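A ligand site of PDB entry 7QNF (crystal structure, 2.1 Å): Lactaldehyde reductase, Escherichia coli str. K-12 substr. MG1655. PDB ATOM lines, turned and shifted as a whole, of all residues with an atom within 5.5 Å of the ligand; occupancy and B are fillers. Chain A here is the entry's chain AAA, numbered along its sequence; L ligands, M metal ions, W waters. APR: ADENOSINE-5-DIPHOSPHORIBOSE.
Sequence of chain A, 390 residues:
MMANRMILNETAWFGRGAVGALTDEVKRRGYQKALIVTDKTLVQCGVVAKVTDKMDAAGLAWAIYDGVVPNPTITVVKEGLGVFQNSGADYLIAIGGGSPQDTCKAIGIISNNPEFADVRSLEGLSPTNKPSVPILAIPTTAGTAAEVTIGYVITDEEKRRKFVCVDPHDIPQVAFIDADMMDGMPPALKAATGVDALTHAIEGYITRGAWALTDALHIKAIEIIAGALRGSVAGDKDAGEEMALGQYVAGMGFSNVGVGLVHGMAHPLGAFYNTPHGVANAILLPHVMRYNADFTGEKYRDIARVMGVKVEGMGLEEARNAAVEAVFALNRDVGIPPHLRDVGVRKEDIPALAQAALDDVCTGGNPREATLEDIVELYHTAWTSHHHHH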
ATOM      1  N   ASP A  39     -18.731  12.645   6.827  1.00  0.00           N
ATOM      2  CA  ASP A  39     -18.790  11.189   7.161  1.00  0.00           C
ATOM      3  C   ASP A  39     -18.600  10.337   5.884  1.00  0.00           C
ATOM      4  O   ASP A  39     -18.729  10.885   4.767  1.00  0.00           O
ATOM      5  CB  ASP A  39     -20.052  10.871   7.974  1.00  0.00           C
ATOM      6  CG  ASP A  39     -21.374  11.045   7.249  1.00  0.00           C
ATOM      7  OD1 ASP A  39     -21.458  10.588   6.117  1.00  0.00           O
ATOM      8  OD2 ASP A  39     -22.293  11.640   7.844  1.00  0.00           O
ATOM      9  N   THR A  41     -20.257   8.035   4.290  1.00  0.00           N
ATOM     10  CA  THR A  41     -21.399   7.975   3.345  1.00  0.00           C
ATOM     11  C   THR A  41     -21.354   9.175   2.414  1.00  0.00           C
ATOM     12  O   THR A  41     -21.396   8.975   1.181  1.00  0.00           O
ATOM     13  CB  THR A  41     -22.733   7.948   4.081  1.00  0.00           C
ATOM     14  OG1 THR A  41     -22.784   6.748   4.835  1.00  0.00           O
ATOM     15  CG2 THR A  41     -23.911   8.013   3.120  1.00  0.00           C
ATOM     16  N   LEU A  42     -21.277  10.389   2.967  1.00  0.00           N
ATOM     17  CA  LEU A  42     -21.356  11.644   2.187  1.00  0.00           C
ATOM     18  C   LEU A  42     -20.169  11.725   1.215  1.00  0.00           C
ATOM     19  O   LEU A  42     -20.352  12.332   0.147  1.00  0.00           O
ATOM     20  CB  LEU A  42     -21.413  12.852   3.121  1.00  0.00           C
ATOM     21  CG  LEU A  42     -22.712  12.996   3.923  1.00  0.00           C
ATOM     22  CD1 LEU A  42     -22.581  14.101   4.961  1.00  0.00           C
ATOM     23  CD2 LEU A  42     -23.898  13.279   3.012  1.00  0.00           C
ATOM     24  N   CYS A  45     -20.918   8.787  -1.556  1.00  0.00           N
ATOM     25  CA  CYS A  45     -22.147   9.160  -2.300  1.00  0.00           C
ATOM     26  C   CYS A  45     -21.879  10.334  -3.260  1.00  0.00           C
ATOM     27  O   CYS A  45     -22.784  10.663  -4.021  1.00  0.00           O
ATOM     28  CB  CYS A  45     -23.317   9.493  -1.357  1.00  0.00           C
ATOM     29  SG  CYS A  45     -24.255   8.037  -0.828  1.00  0.00           S
ATOM     30  N   VAL A  47     -21.528  13.532  -2.500  1.00  0.00           N
ATOM     31  CA  VAL A  47     -22.056  14.816  -1.958  1.00  0.00           C
ATOM     32  C   VAL A  47     -20.885  15.745  -1.615  1.00  0.00           C
ATOM     33  O   VAL A  47     -20.940  16.928  -2.006  1.00  0.00           O
ATOM     34  CB  VAL A  47     -22.994  14.574  -0.753  1.00  0.00           C
ATOM     35  CG1 VAL A  47     -23.399  15.883  -0.099  1.00  0.00           C
ATOM     36  CG2 VAL A  47     -24.235  13.768  -1.142  1.00  0.00           C
ATOM     37  N   VAL A  69     -19.248   9.543  13.027  1.00  0.00           N
ATOM     38  CA  VAL A  69     -20.356   8.541  13.053  1.00  0.00           C
ATOM     39  C   VAL A  69     -21.578   9.201  13.687  1.00  0.00           C
ATOM     40  O   VAL A  69     -21.430  10.132  14.473  1.00  0.00           O
ATOM     41  CB  VAL A  69     -20.001   7.235  13.797  1.00  0.00           C
ATOM     42  CG1 VAL A  69     -19.050   6.385  12.989  1.00  0.00           C
ATOM     43  CG2 VAL A  69     -19.469   7.483  15.205  1.00  0.00           C
ATOM     44  N   PRO A  70     -22.800   8.718  13.365  1.00  0.00           N
ATOM     45  CA  PRO A  70     -24.032   9.234  13.966  1.00  0.00           C
ATOM     46  C   PRO A  70     -23.954   9.230  15.502  1.00  0.00           C
ATOM     47  O   PRO A  70     -23.384   8.302  16.050  1.00  0.00           O
ATOM     48  CB  PRO A  70     -25.104   8.254  13.482  1.00  0.00           C
ATOM     49  CG  PRO A  70     -24.559   7.746  12.173  1.00  0.00           C
ATOM     50  CD  PRO A  70     -23.067   7.641  12.396  1.00  0.00           C
ATOM     51  N   ASN A  71     -24.476  10.274  16.144  1.00  0.00           N
ATOM     52  CA  ASN A  71     -24.334  10.510  17.603  1.00  0.00           C
ATOM     53  C   ASN A  71     -22.838  10.565  17.898  1.00  0.00           C
ATOM     54  O   ASN A  71     -22.309   9.719  18.620  1.00  0.00           O
ATOM     55  CB  ASN A  71     -25.078   9.447  18.425  1.00  0.00           C
ATOM     56  CG  ASN A  71     -26.523   9.301  18.008  1.00  0.00           C
ATOM     57  OD1 ASN A  71     -26.985   8.193  17.703  1.00  0.00           O
ATOM     58  ND2 ASN A  71     -27.259  10.392  17.994  1.00  0.00           N
ATOM     59  N   PRO A  72     -22.118  11.571  17.347  1.00  0.00           N
ATOM     60  CA  PRO A  72     -20.656  11.629  17.409  1.00  0.00           C
ATOM     61  C   PRO A  72     -20.151  11.564  18.845  1.00  0.00           C
ATOM     62  O   PRO A  72     -20.784  12.142  19.721  1.00  0.00           O
ATOM     63  CB  PRO A  72     -20.291  12.984  16.794  1.00  0.00           C
ATOM     64  CG  PRO A  72     -21.582  13.775  16.893  1.00  0.00           C
ATOM     65  CD  PRO A  72     -22.667  12.752  16.664  1.00  0.00           C
ATOM     66  N   GLY A  96     -22.504  17.931   6.216  1.00  0.00           N
ATOM     67  CA  GLY A  96     -23.335  16.787   6.624  1.00  0.00           C
ATOM     68  C   GLY A  96     -24.501  17.203   7.494  1.00  0.00           C
ATOM     69  O   GLY A  96     -24.872  18.385   7.466  1.00  0.00           O
ATOM     70  N   GLY A  97     -25.057  16.243   8.229  1.00  0.00           N
ATOM     71  CA  GLY A  97     -26.123  16.489   9.210  1.00  0.00           C
ATOM     72  C   GLY A  97     -25.551  16.962  10.525  1.00  0.00           C
ATOM     73  O   GLY A  97     -24.378  17.411  10.552  1.00  0.00           O
ATOM     74  N   GLY A  98     -26.359  16.884  11.581  1.00  0.00           N
ATOM     75  CA  GLY A  98     -25.983  17.277  12.949  1.00  0.00           C
ATOM     76  C   GLY A  98     -24.691  16.624  13.395  1.00  0.00           C
ATOM     77  O   GLY A  98     -23.910  17.288  14.084  1.00  0.00           O
ATOM     78  N   SER A  99     -24.459  15.363  13.034  1.00  0.00           N
ATOM     79  CA  SER A  99     -23.297  14.583  13.547  1.00  0.00           C
ATOM     80  C   SER A  99     -21.988  15.217  13.063  1.00  0.00           C
ATOM     81  O   SER A  99     -21.147  15.611  13.888  1.00  0.00           O
ATOM     82  CB  SER A  99     -23.433  13.100  13.243  1.00  0.00           C
ATOM     83  OG  SER A  99     -24.523  12.548  13.980  1.00  0.00           O
ATOM     84  N   PRO A 100     -21.731  15.347  11.740  1.00  0.00           N
ATOM     85  CA  PRO A 100     -20.561  16.066  11.269  1.00  0.00           C
ATOM     86  C   PRO A 100     -20.508  17.537  11.728  1.00  0.00           C
ATOM     87  O   PRO A 100     -19.457  17.984  12.124  1.00  0.00           O
ATOM     88  CB  PRO A 100     -20.668  15.955   9.736  1.00  0.00           C
ATOM     89  CG  PRO A 100     -21.489  14.715   9.506  1.00  0.00           C
ATOM     90  CD  PRO A 100     -22.478  14.687  10.648  1.00  0.00           C
ATOM     91  N   ASP A 102     -21.930  19.071  14.479  1.00  0.00           N
ATOM     92  CA  ASP A 102     -21.638  19.141  15.936  1.00  0.00           C
ATOM     93  C   ASP A 102     -20.151  18.817  16.157  1.00  0.00           C
ATOM     94  O   ASP A 102     -19.515  19.524  16.968  1.00  0.00           O
ATOM     95  CB  ASP A 102     -22.584  18.250  16.742  1.00  0.00           C
ATOM     96  CG  ASP A 102     -24.011  18.782  16.774  1.00  0.00           C
ATOM     97  OD1 ASP A 102     -24.253  19.826  16.120  1.00  0.00           O
ATOM     98  OD2 ASP A 102     -24.855  18.156  17.451  1.00  0.00           O
ATOM     99  N   THR A 140     -26.616  18.614   4.977  1.00  0.00           N
ATOM    100  CA  THR A 140     -27.022  17.557   4.017  1.00  0.00           C
ATOM    101  C   THR A 140     -28.264  16.831   4.523  1.00  0.00           C
ATOM    102  O   THR A 140     -28.727  15.903   3.815  1.00  0.00           O
ATOM    103  CB  THR A 140     -25.863  16.578   3.747  1.00  0.00           C
ATOM    104  OG1 THR A 140     -25.689  15.779   4.913  1.00  0.00           O
ATOM    105  CG2 THR A 140     -24.572  17.279   3.366  1.00  0.00           C
ATOM    106  N   THR A 141     -28.827  17.219   5.683  1.00  0.00           N
ATOM    107  CA  THR A 141     -30.132  16.698   6.180  1.00  0.00           C
ATOM    108  C   THR A 141     -31.075  17.862   6.397  1.00  0.00           C
ATOM    109  O   THR A 141     -30.591  18.978   6.532  1.00  0.00           O
ATOM    110  CB  THR A 141     -30.019  15.839   7.439  1.00  0.00           C
ATOM    111  OG1 THR A 141     -29.526  16.622   8.525  1.00  0.00           O
ATOM    112  CG2 THR A 141     -29.162  14.617   7.207  1.00  0.00           C
ATOM    113  N   GLY A 143     -33.249  18.831   8.709  1.00  0.00           N
ATOM    114  CA  GLY A 143     -33.076  18.212  10.022  1.00  0.00           C
ATOM    115  C   GLY A 143     -32.663  19.204  11.075  1.00  0.00           C
ATOM    116  O   GLY A 143     -33.543  19.914  11.551  1.00  0.00           O
ATOM    117  N   THR A 144     -31.370  19.227  11.438  1.00  0.00           N
ATOM    118  CA  THR A 144     -30.918  19.632  12.795  1.00  0.00           C
ATOM    119  C   THR A 144     -30.747  21.151  12.930  1.00  0.00           C
ATOM    120  O   THR A 144     -30.763  21.631  14.086  1.00  0.00           O
ATOM    121  CB  THR A 144     -29.618  18.908  13.216  1.00  0.00           C
ATOM    122  OG1 THR A 144     -28.521  19.474  12.512  1.00  0.00           O
ATOM    123  CG2 THR A 144     -29.717  17.403  13.041  1.00  0.00           C
ATOM    124  N   VAL A 153     -24.201  18.472  20.269  1.00  0.00           N
ATOM    125  CA  VAL A 153     -24.428  17.275  21.146  1.00  0.00           C
ATOM    126  C   VAL A 153     -23.361  16.208  20.841  1.00  0.00           C
ATOM    127  O   VAL A 153     -23.254  15.714  19.687  1.00  0.00           O
ATOM    128  CB  VAL A 153     -25.860  16.726  20.994  1.00  0.00           C
ATOM    129  CG1 VAL A 153     -26.186  15.701  22.069  1.00  0.00           C
ATOM    130  CG2 VAL A 153     -26.886  17.841  21.015  1.00  0.00           C
ATOM    131  N   LYS A 162     -25.460  11.459  26.184  1.00  0.00           N
ATOM    132  CA  LYS A 162     -25.290  12.570  25.221  1.00  0.00           C
ATOM    133  C   LYS A 162     -25.278  13.848  26.058  1.00  0.00           C
ATOM    134  O   LYS A 162     -26.114  13.938  26.975  1.00  0.00           O
ATOM    135  CB  LYS A 162     -26.409  12.566  24.166  1.00  0.00           C
ATOM    136  CG  LYS A 162     -26.079  11.769  22.907  1.00  0.00           C
ATOM    137  CD  LYS A 162     -27.269  11.377  22.049  1.00  0.00           C
ATOM    138  CE  LYS A 162     -27.719  12.452  21.090  1.00  0.00           C
ATOM    139  NZ  LYS A 162     -26.781  12.598  19.957  1.00  0.00           N
ATOM    140  N   MET A 181     -27.675  19.419  -1.932  1.00  0.00           N
ATOM    141  CA  MET A 181     -26.820  18.629  -1.004  1.00  0.00           C
ATOM    142  C   MET A 181     -27.684  17.632  -0.212  1.00  0.00           C
ATOM    143  O   MET A 181     -27.114  16.726   0.428  1.00  0.00           O
ATOM    144  CB  MET A 181     -26.094  19.555  -0.026  1.00  0.00           C
ATOM    145  CG  MET A 181     -25.271  20.638  -0.688  1.00  0.00           C
ATOM    146  SD  MET A 181     -23.880  19.962  -1.641  1.00  0.00           S
ATOM    147  CE  MET A 181     -22.799  19.365  -0.336  1.00  0.00           C
ATOM    148  N   MET A 182     -29.016  17.778  -0.276  1.00  0.00           N
ATOM    149  CA  MET A 182     -29.987  17.054   0.583  1.00  0.00           C
ATOM    150  C   MET A 182     -30.704  15.923  -0.186  1.00  0.00           C
ATOM    151  O   MET A 182     -31.148  14.950   0.469  1.00  0.00           O
ATOM    152  CB  MET A 182     -31.027  18.040   1.123  1.00  0.00           C
ATOM    153  CG  MET A 182     -30.474  18.853   2.271  1.00  0.00           C
ATOM    154  SD  MET A 182     -31.419  20.324   2.650  1.00  0.00           S
ATOM    155  CE  MET A 182     -30.282  21.147   3.753  1.00  0.00           C
ATOM    156  N   ASP A 183     -30.803  16.051  -1.514  1.00  0.00           N
ATOM    157  CA  ASP A 183     -31.639  15.174  -2.384  1.00  0.00           C
ATOM    158  C   ASP A 183     -31.252  13.710  -2.246  1.00  0.00           C
ATOM    159  O   ASP A 183     -32.116  12.881  -2.519  1.00  0.00           O
ATOM    160  CB  ASP A 183     -31.538  15.579  -3.856  1.00  0.00           C
ATOM    161  CG  ASP A 183     -32.206  16.909  -4.159  1.00  0.00           C
ATOM    162  OD1 ASP A 183     -33.198  17.224  -3.488  1.00  0.00           O
ATOM    163  OD2 ASP A 183     -31.714  17.619  -5.038  1.00  0.00           O
ATOM    164  N   GLY A 184     -30.021  13.393  -1.852  1.00  0.00           N
ATOM    165  CA  GLY A 184     -29.541  11.993  -1.727  1.00  0.00           C
ATOM    166  C   GLY A 184     -30.109  11.291  -0.503  1.00  0.00           C
ATOM    167  O   GLY A 184     -30.009  10.051  -0.450  1.00  0.00           O
ATOM    168  N   MET A 185     -30.660  12.047   0.458  1.00  0.00           N
ATOM    169  CA  MET A 185     -31.283  11.476   1.691  1.00  0.00           C
ATOM    170  C   MET A 185     -32.269  10.365   1.321  1.00  0.00           C
ATOM    171  O   MET A 185     -33.243  10.619   0.621  1.00  0.00           O
ATOM    172  CB  MET A 185     -32.053  12.542   2.458  1.00  0.00           C
ATOM    173  CG  MET A 185     -31.211  13.339   3.403  1.00  0.00           C
ATOM    174  SD  MET A 185     -32.242  14.199   4.607  1.00  0.00           S
ATOM    175  CE  MET A 185     -32.851  15.574   3.641  1.00  0.00           C
ATOM    176  N   PRO A 186     -32.073   9.100   1.766  1.00  0.00           N
ATOM    177  CA  PRO A 186     -33.118   8.087   1.657  1.00  0.00           C
ATOM    178  C   PRO A 186     -34.442   8.595   2.244  1.00  0.00           C
ATOM    179  O   PRO A 186     -34.447   9.434   3.141  1.00  0.00           O
ATOM    180  CB  PRO A 186     -32.530   6.916   2.461  1.00  0.00           C
ATOM    181  CG  PRO A 186     -31.038   7.068   2.266  1.00  0.00           C
ATOM    182  CD  PRO A 186     -30.823   8.570   2.341  1.00  0.00           C
ATOM    183  N   LEU A 189     -34.641   8.752   6.021  1.00  0.00           N
ATOM    184  CA  LEU A 189     -33.783   9.831   6.578  1.00  0.00           C
ATOM    185  C   LEU A 189     -34.478  11.194   6.450  1.00  0.00           C
ATOM    186  O   LEU A 189     -34.379  12.026   7.406  1.00  0.00           O
ATOM    187  CB  LEU A 189     -32.433   9.816   5.868  1.00  0.00           C
ATOM    188  CG  LEU A 189     -31.394  10.812   6.376  1.00  0.00           C
ATOM    189  CD1 LEU A 189     -31.160  10.663   7.871  1.00  0.00           C
ATOM    190  CD2 LEU A 189     -30.075  10.654   5.635  1.00  0.00           C
ATOM    191  N   THR A 193     -35.282  13.212   9.860  1.00  0.00           N
ATOM    192  CA  THR A 193     -34.694  14.570  10.045  1.00  0.00           C
ATOM    193  C   THR A 193     -35.810  15.619   9.961  1.00  0.00           C
ATOM    194  O   THR A 193     -35.748  16.606  10.715  1.00  0.00           O
ATOM    195  CB  THR A 193     -33.507  14.791   9.104  1.00  0.00           C
ATOM    196  OG1 THR A 193     -33.943  14.812   7.748  1.00  0.00           O
ATOM    197  CG2 THR A 193     -32.429  13.746   9.325  1.00  0.00           C
ATOM    198  N   ASP A 196     -37.542  15.612  13.343  1.00  0.00           N
ATOM    199  CA  ASP A 196     -36.590  16.326  14.218  1.00  0.00           C
ATOM    200  C   ASP A 196     -36.823  17.830  14.063  1.00  0.00           C
ATOM    201  O   ASP A 196     -36.958  18.512  15.103  1.00  0.00           O
ATOM    202  CB  ASP A 196     -35.135  15.908  13.955  1.00  0.00           C
ATOM    203  CG  ASP A 196     -34.110  16.568  14.866  1.00  0.00           C
ATOM    204  OD1 ASP A 196     -34.433  16.847  16.068  1.00  0.00           O
ATOM    205  OD2 ASP A 196     -32.970  16.791  14.370  1.00  0.00           O
ATOM    206  N   HIS A 267     -32.423  12.011  23.904  1.00  0.00           N
ATOM    207  CA  HIS A 267     -30.946  11.991  24.043  1.00  0.00           C
ATOM    208  C   HIS A 267     -30.478  10.701  24.712  1.00  0.00           C
ATOM    209  O   HIS A 267     -29.552  10.068  24.215  1.00  0.00           O
ATOM    210  CB  HIS A 267     -30.430  13.260  24.754  1.00  0.00           C
ATOM    211  CG  HIS A 267     -30.383  14.444  23.835  1.00  0.00           C
ATOM    212  ND1 HIS A 267     -30.277  15.752  24.294  1.00  0.00           N
ATOM    213  CD2 HIS A 267     -30.465  14.504  22.484  1.00  0.00           C
ATOM    214  CE1 HIS A 267     -30.276  16.562  23.265  1.00  0.00           C
ATOM    215  NE2 HIS A 267     -30.400  15.821  22.135  1.00  0.00           N
ATOM    216  N   HIS A 277     -31.698  10.207  16.153  1.00  0.00           N
ATOM    217  CA  HIS A 277     -32.247  11.288  17.008  1.00  0.00           C
ATOM    218  C   HIS A 277     -33.673  11.677  16.568  1.00  0.00           C
ATOM    219  O   HIS A 277     -34.534  11.921  17.440  1.00  0.00           O
ATOM    220  CB  HIS A 277     -31.219  12.436  16.982  1.00  0.00           C
ATOM    221  CG  HIS A 277     -31.714  13.715  17.531  1.00  0.00           C
ATOM    222  ND1 HIS A 277     -31.833  13.947  18.872  1.00  0.00           N
ATOM    223  CD2 HIS A 277     -32.117  14.837  16.898  1.00  0.00           C
ATOM    224  CE1 HIS A 277     -32.306  15.155  19.068  1.00  0.00           C
ATOM    225  NE2 HIS A 277     -32.476  15.734  17.867  1.00  0.00           N
ATOM    226  N   GLY A 278     -33.912  11.746  15.265  1.00  0.00           N
ATOM    227  CA  GLY A 278     -35.217  12.144  14.692  1.00  0.00           C
ATOM    228  C   GLY A 278     -36.267  11.066  14.871  1.00  0.00           C
ATOM    229  O   GLY A 278     -37.428  11.416  15.093  1.00  0.00           O
HETATM  230  N1  APR L   1     -27.704  11.466   1.636  1.00  0.00           N
HETATM  231  C2  APR L   1     -27.555  10.256   2.190  1.00  0.00           C
HETATM  232  N3  APR L   1     -27.236   9.941   3.447  1.00  0.00           N
HETATM  233  C4  APR L   1     -27.057  11.054   4.182  1.00  0.00           C
HETATM  234  C5  APR L   1     -27.184  12.356   3.759  1.00  0.00           C
HETATM  235  C6  APR L   1     -27.520  12.569   2.407  1.00  0.00           C
HETATM  236  N6  APR L   1     -27.677  13.768   1.856  1.00  0.00           N
HETATM  237  N7  APR L   1     -26.926  13.219   4.814  1.00  0.00           N
HETATM  238  C8  APR L   1     -26.642  12.441   5.831  1.00  0.00           C
HETATM  239  N9  APR L   1     -26.728  11.119   5.514  1.00  0.00           N
HETATM  240  C1' APR L   1     -26.474   9.983   6.390  1.00  0.00           C
HETATM  241  C2' APR L   1     -25.170  10.091   7.166  1.00  0.00           C
HETATM  242  O2' APR L   1     -24.064   9.658   6.412  1.00  0.00           O
HETATM  243  C3' APR L   1     -25.453   9.134   8.321  1.00  0.00           C
HETATM  244  O3' APR L   1     -25.094   7.816   7.919  1.00  0.00           O
HETATM  245  O4' APR L   1     -27.481   9.919   7.360  1.00  0.00           O
HETATM  246  C4' APR L   1     -26.964   9.302   8.566  1.00  0.00           C
HETATM  247  C5' APR L   1     -27.334  10.144   9.758  1.00  0.00           C
HETATM  248  O5' APR L   1     -26.523  11.341   9.759  1.00  0.00           O
HETATM  249  PA  APR L   1     -26.491  12.307  11.038  1.00  0.00           P
HETATM  250  O1A APR L   1     -25.541  13.434  10.772  1.00  0.00           O
HETATM  251  O2A APR L   1     -26.282  11.483  12.266  1.00  0.00           O
HETATM  252  O3A APR L   1     -27.999  12.852  11.033  1.00  0.00           O
HETATM  253  PB  APR L   1     -28.761  14.152  11.577  1.00  0.00           P
HETATM  254  O1B APR L   1     -28.650  15.247  10.569  1.00  0.00           O
HETATM  255  O2B APR L   1     -30.133  13.757  12.014  1.00  0.00           O
HETATM  256  O5D APR L   1     -27.875  14.511  12.869  1.00  0.00           O
HETATM  257  C5D APR L   1     -28.169  13.870  14.134  1.00  0.00           C
HETATM  258  O4D APR L   1     -27.448  15.833  15.339  1.00  0.00           O
HETATM  259  O1D APR L   1     -28.691  17.187  16.740  1.00  0.00           O
HETATM  260  C1D APR L   1     -27.773  16.157  16.694  1.00  0.00           C
HETATM  261  O2D APR L   1     -28.346  14.752  18.678  1.00  0.00           O
HETATM  262  C2D APR L   1     -28.353  14.866  17.272  1.00  0.00           C
HETATM  263  O3D APR L   1     -26.241  13.604  17.296  1.00  0.00           O
HETATM  264  C3D APR L   1     -27.468  13.813  16.620  1.00  0.00           C
HETATM  265  C4D APR L   1     -27.250  14.411  15.214  1.00  0.00           C
HETATM  266 FE    FE M   1     -32.936  17.829  17.534  1.00  0.00          FE
HETATM  267  O   HOH W   1     -24.280  13.461   8.250  1.00  0.00           O
HETATM  268  O   HOH W   2     -29.706  16.707  19.884  1.00  0.00           O
HETATM  269  O   HOH W   3     -27.642  14.360  -1.052  1.00  0.00           O
HETATM  270  O   HOH W   4     -31.333  17.770  16.234  1.00  0.00           O
HETATM  271  O   HOH W   5     -22.321   7.441   8.460  1.00  0.00           O
HETATM  272  O   HOH W   6     -24.564  15.501  17.277  1.00  0.00           O
HETATM  273  O   HOH W   7     -27.314  19.439  16.964  1.00  0.00           O
HETATM  274  O   HOH W   8     -32.296  14.761  12.786  1.00  0.00           O
HETATM  275  O   HOH W   9     -27.772   7.337   4.090  1.00  0.00           O
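O of Gly 184 sits close to N1 of the ligand (3.4 Å).
Thr 41 touches the ligand (CB to O2', 3.2 Å).
CD2 of Leu 42 touches C5 of the ligand (3.5 Å).
Pro 70 touches the ligand.
Pro 72 touches the ligand (CD to O3D, 3.7 Å).
Gly 97 touches the ligand.
CD of Pro 100 touches O1A of the ligand, 3.3 Å away.
Asp 102 touches the ligand (OD2 to C1D, 3.6 Å).
CG2 of Thr 144 touches O5D of the ligand (3.4 Å).
Val 153 touches the ligand (CB to O2D, 3.9 Å).
O of Met 182 touches N6 of the ligand, at 3.9 Å.
CD of Pro 186 touches C2 of the ligand, 3.7 Å away.
Leu 189 touches the ligand.
CG2 of Thr 193 touches O2B of the ligand (3.5 Å).
CG of His 277 touches C2D of the ligand (3.6 Å).
Hydrophobic or aromatic side chains within 4 Å of the ligand: Leu 42, Pro 70, Pro 72, Pro 100, Val 153, Met 185, Pro 186, Leu 189 and His 277.
Of the 33 residues printed, 24 come within 4 Å of the ligand.
The nearest printed residue that does not touch the ligand is His 267 (4.2 Å).
Water W8 lies within hydrogen-bond range of an oxygen (O2B) of the ligand (2.5 Å) and the side-chain carboxylate of Asp 196 (2.7 Å).
Water W6 lies within hydrogen-bond range of O3D of the ligand, OD2 of Asp 102 and O of Val 153.
Water W7 lies within hydrogen-bond range of O1D of the ligand and OD2 of Asp 102.
Water W4 bridges OD2 of Asp 196 (2.7 Å) and O1D of the ligand (2.8 Å).
Water W1 lies within hydrogen-bond range of OD2 of Asp 39, O1A of the ligand and N of Gly 97.
Water W3 lies within hydrogen-bond range of N of Gly 184 (2.7 Å), O of Met 181 (2.8 Å) and N6 of the ligand (3.0 Å).
The side-chain hydroxyl of Thr 141 sits at hydrogen-bond distance from an oxygen (O1B) of the ligand (2.6 Å).
N of Ser 99 sits at hydrogen-bond distance from O1A of the ligand, at 3.2 Å.
O2A of the ligand lies within hydrogen-bond range of OG of Ser 99, at 2.7 Å.
The side-chain carboxylate of Asp 39 lies within hydrogen-bond range of an oxygen (O2') of the ligand.
The backbone carbonyl oxygen (O) of Thr 140 is in hydrogen-bond range of a nitrogen (N6) of the ligand (3.1 Å).
The side-chain hydroxyl (OG1) of Thr 140 sits at hydrogen-bond distance from a nitrogen (N7) of the ligand (2.8 Å).
The side-chain amino group (NZ) of Lys 162 lies within hydrogen-bond range of an oxygen (O3D) of the ligand (2.9 Å).
N of Gly 98 lies within hydrogen-bond range of O1B of the ligand (3.0 Å).
The backbone NH (N) of Met 185 sits at hydrogen-bond distance from a nitrogen (N1) of the ligand, at 3.2 Å.
The backbone carbonyl oxygen (O) of Met 181 is in hydrogen-bond range of a nitrogen (N6) of the ligand, at 3.3 Å.
The side-chain amide nitrogen (ND2) of Asn 71 sits at hydrogen-bond distance from an oxygen (O3D) of the ligand, at 3.4 Å.
OD1 of Asp 39 sits close to N of Thr 41 (3.4 Å).
The backbone NH of Thr 140 sits at hydrogen-bond distance from the backbone carbonyl oxygen of Gly 96, at 3.0 Å.
NZ of Lys 162 lies close to ND2 of Asn 71 (3.0 Å).
The backbone NH (N) of Gly 98 lies close to the side-chain hydroxyl (OG1) of Thr 144 (3.5 Å).
SG of Cys 45 sits close to O of Thr 41 (3.6 Å).
The side-chain sulfur (SD) of Met 185 lies within hydrogen-bond range of the side-chain hydroxyl (OG1) of Thr 193, 3.6 Å away.
O of Leu 42 lies within hydrogen-bond range of N of Val 47.
The side-chain carboxylate (OD2) of Asp 102 is in hydrogen-bond range of the backbone NH (N) of Val 153 (2.9 Å).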
